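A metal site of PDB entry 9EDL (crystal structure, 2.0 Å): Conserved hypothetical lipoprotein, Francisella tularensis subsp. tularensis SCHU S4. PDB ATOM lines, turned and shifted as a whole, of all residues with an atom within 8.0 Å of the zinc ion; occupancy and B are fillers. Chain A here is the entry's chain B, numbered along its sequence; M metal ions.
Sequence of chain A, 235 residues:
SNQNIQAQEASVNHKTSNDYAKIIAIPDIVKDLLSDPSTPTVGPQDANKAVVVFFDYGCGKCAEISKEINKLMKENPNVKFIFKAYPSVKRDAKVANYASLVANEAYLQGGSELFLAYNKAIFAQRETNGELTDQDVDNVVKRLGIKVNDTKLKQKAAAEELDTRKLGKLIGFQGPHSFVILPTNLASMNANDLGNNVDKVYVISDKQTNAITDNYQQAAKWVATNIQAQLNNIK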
ATOM      1  N   GLY A  60       0.536  27.716 -10.218  1.00  0.00           N
ATOM      2  CA  GLY A  60       0.023  27.080  -9.026  1.00  0.00           C
ATOM      3  C   GLY A  60       0.784  25.837  -8.629  1.00  0.00           C
ATOM      4  O   GLY A  60       0.895  25.522  -7.446  1.00  0.00           O
ATOM      5  N   ALA A  63       3.730  26.961  -6.770  1.00  0.00           N
ATOM      6  CA  ALA A  63       3.366  27.443  -5.446  1.00  0.00           C
ATOM      7  C   ALA A  63       3.298  26.295  -4.445  1.00  0.00           C
ATOM      8  O   ALA A  63       3.655  26.457  -3.277  1.00  0.00           O
ATOM      9  CB  ALA A  63       2.032  28.198  -5.497  1.00  0.00           C
ATOM     10  N   GLU A  64       2.882  25.122  -4.917  1.00  0.00           N
ATOM     11  CA  GLU A  64       2.803  23.943  -4.068  1.00  0.00           C
ATOM     12  C   GLU A  64       4.180  23.304  -3.892  1.00  0.00           C
ATOM     13  O   GLU A  64       4.564  22.933  -2.775  1.00  0.00           O
ATOM     14  CB  GLU A  64       1.790  22.964  -4.667  1.00  0.00           C
ATOM     15  CG  GLU A  64       1.108  22.041  -3.655  1.00  0.00           C
ATOM     16  CD  GLU A  64       0.346  22.801  -2.578  1.00  0.00           C
ATOM     17  OE1 GLU A  64      -0.585  23.574  -2.904  1.00  0.00           O
ATOM     18  OE2 GLU A  64       0.690  22.622  -1.391  1.00  0.00           O
ATOM     19  N   ILE A  65       4.945  23.206  -4.978  1.00  0.00           N
ATOM     20  CA  ILE A  65       6.340  22.765  -4.901  1.00  0.00           C
ATOM     21  C   ILE A  65       7.116  23.597  -3.885  1.00  0.00           C
ATOM     22  O   ILE A  65       7.898  23.066  -3.085  1.00  0.00           O
ATOM     23  CB  ILE A  65       6.972  22.824  -6.302  1.00  0.00           C
ATOM     24  CG1 ILE A  65       6.323  21.759  -7.197  1.00  0.00           C
ATOM     25  CG2 ILE A  65       8.476  22.672  -6.219  1.00  0.00           C
ATOM     26  CD1 ILE A  65       6.687  21.848  -8.650  1.00  0.00           C
ATOM     27  N   LYS A  67       6.283  24.889  -1.116  1.00  0.00           N
ATOM     28  CA  LYS A  67       6.121  24.480   0.270  1.00  0.00           C
ATOM     29  C   LYS A  67       6.877  23.195   0.574  1.00  0.00           C
ATOM     30  O   LYS A  67       7.402  23.032   1.681  1.00  0.00           O
ATOM     31  CB  LYS A  67       4.634  24.335   0.598  1.00  0.00           C
ATOM     32  CG  LYS A  67       4.004  25.692   0.886  1.00  0.00           C
ATOM     33  CD  LYS A  67       2.607  25.826   0.301  1.00  0.00           C
ATOM     34  CE  LYS A  67       1.638  24.851   0.911  1.00  0.00           C
ATOM     35  NZ  LYS A  67       0.271  25.177   0.419  1.00  0.00           N
ATOM     36  N   PHE A 123       3.984  33.424  -3.259  1.00  0.00           N
ATOM     37  CA  PHE A 123       3.420  32.131  -3.611  1.00  0.00           C
ATOM     38  C   PHE A 123       2.116  31.885  -2.863  1.00  0.00           C
ATOM     39  O   PHE A 123       1.179  31.317  -3.422  1.00  0.00           O
ATOM     40  CB  PHE A 123       4.424  31.023  -3.310  1.00  0.00           C
ATOM     41  CG  PHE A 123       5.310  30.675  -4.475  1.00  0.00           C
ATOM     42  CD1 PHE A 123       4.782  30.456  -5.733  1.00  0.00           C
ATOM     43  CD2 PHE A 123       6.684  30.543  -4.304  1.00  0.00           C
ATOM     44  CE1 PHE A 123       5.614  30.099  -6.802  1.00  0.00           C
ATOM     45  CE2 PHE A 123       7.516  30.192  -5.365  1.00  0.00           C
ATOM     46  CZ  PHE A 123       6.982  29.970  -6.596  1.00  0.00           C
ATOM     47  N   ALA A 124       2.036  32.346  -1.606  1.00  0.00           N
ATOM     48  CA  ALA A 124       0.783  32.197  -0.858  1.00  0.00           C
ATOM     49  C   ALA A 124      -0.348  32.964  -1.525  1.00  0.00           C
ATOM     50  O   ALA A 124      -1.500  32.497  -1.554  1.00  0.00           O
ATOM     51  CB  ALA A 124       0.973  32.686   0.583  1.00  0.00           C
ATOM     52  N   GLU A 127      -1.367  31.011  -4.581  1.00  0.00           N
ATOM     53  CA  GLU A 127      -2.080  29.805  -4.169  1.00  0.00           C
ATOM     54  C   GLU A 127      -3.503  30.150  -3.774  1.00  0.00           C
ATOM     55  O   GLU A 127      -4.464  29.528  -4.242  1.00  0.00           O
ATOM     56  CB  GLU A 127      -1.308  29.158  -3.019  1.00  0.00           C
ATOM     57  CG  GLU A 127      -1.631  27.718  -2.730  1.00  0.00           C
ATOM     58  CD  GLU A 127      -0.551  27.107  -1.891  1.00  0.00           C
ATOM     59  OE1 GLU A 127      -0.137  27.727  -0.880  1.00  0.00           O
ATOM     60  OE2 GLU A 127      -0.065  26.019  -2.265  1.00  0.00           O
ATOM     61  N   THR A 128      -3.674  31.196  -2.965  1.00  0.00           N
ATOM     62  CA  THR A 128      -4.988  31.577  -2.474  1.00  0.00           C
ATOM     63  C   THR A 128      -5.912  32.060  -3.597  1.00  0.00           C
ATOM     64  O   THR A 128      -7.091  31.700  -3.643  1.00  0.00           O
ATOM     65  CB  THR A 128      -4.823  32.647  -1.393  1.00  0.00           C
ATOM     66  OG1 THR A 128      -4.144  32.066  -0.265  1.00  0.00           O
ATOM     67  CG2 THR A 128      -6.159  33.211  -0.939  1.00  0.00           C
ATOM     68  N   TYR A 216      -1.354  19.205  -8.095  1.00  0.00           N
ATOM     69  CA  TYR A 216      -0.242  20.032  -7.635  1.00  0.00           C
ATOM     70  C   TYR A 216       0.415  19.447  -6.404  1.00  0.00           C
ATOM     71  O   TYR A 216       1.648  19.439  -6.296  1.00  0.00           O
ATOM     72  CB  TYR A 216      -0.718  21.454  -7.274  1.00  0.00           C
ATOM     73  CG  TYR A 216      -1.325  22.273  -8.396  1.00  0.00           C
ATOM     74  CD1 TYR A 216      -1.323  21.836  -9.706  1.00  0.00           C
ATOM     75  CD2 TYR A 216      -1.893  23.512  -8.120  1.00  0.00           C
ATOM     76  CE1 TYR A 216      -1.884  22.601 -10.713  1.00  0.00           C
ATOM     77  CE2 TYR A 216      -2.467  24.285  -9.108  1.00  0.00           C
ATOM     78  CZ  TYR A 216      -2.453  23.826 -10.402  1.00  0.00           C
ATOM     79  OH  TYR A 216      -3.021  24.583 -11.390  1.00  0.00           O
ATOM     80  N   GLN A 217      -0.392  18.984  -5.445  1.00  0.00           N
ATOM     81  CA  GLN A 217       0.141  18.545  -4.169  1.00  0.00           C
ATOM     82  C   GLN A 217       1.007  17.303  -4.338  1.00  0.00           C
ATOM     83  O   GLN A 217       2.137  17.249  -3.844  1.00  0.00           O
ATOM     84  CB  GLN A 217      -1.009  18.292  -3.196  1.00  0.00           C
ATOM     85  CG  GLN A 217      -0.593  18.010  -1.784  1.00  0.00           C
ATOM     86  CD  GLN A 217      -1.780  17.929  -0.838  1.00  0.00           C
ATOM     87  OE1 GLN A 217      -2.526  18.906  -0.661  1.00  0.00           O
ATOM     88  NE2 GLN A 217      -1.978  16.756  -0.228  1.00  0.00           N
HETATM   89 ZN    ZN M   1      -1.352  24.692  -1.308  1.00  0.00          ZN
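Within 4 Å of the zinc ion: Glu 64, Lys 67 and Glu 127.
The zinc ion is bound by OE2 of Glu 127, OE1 of Glu 64 and NZ of Lys 67.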
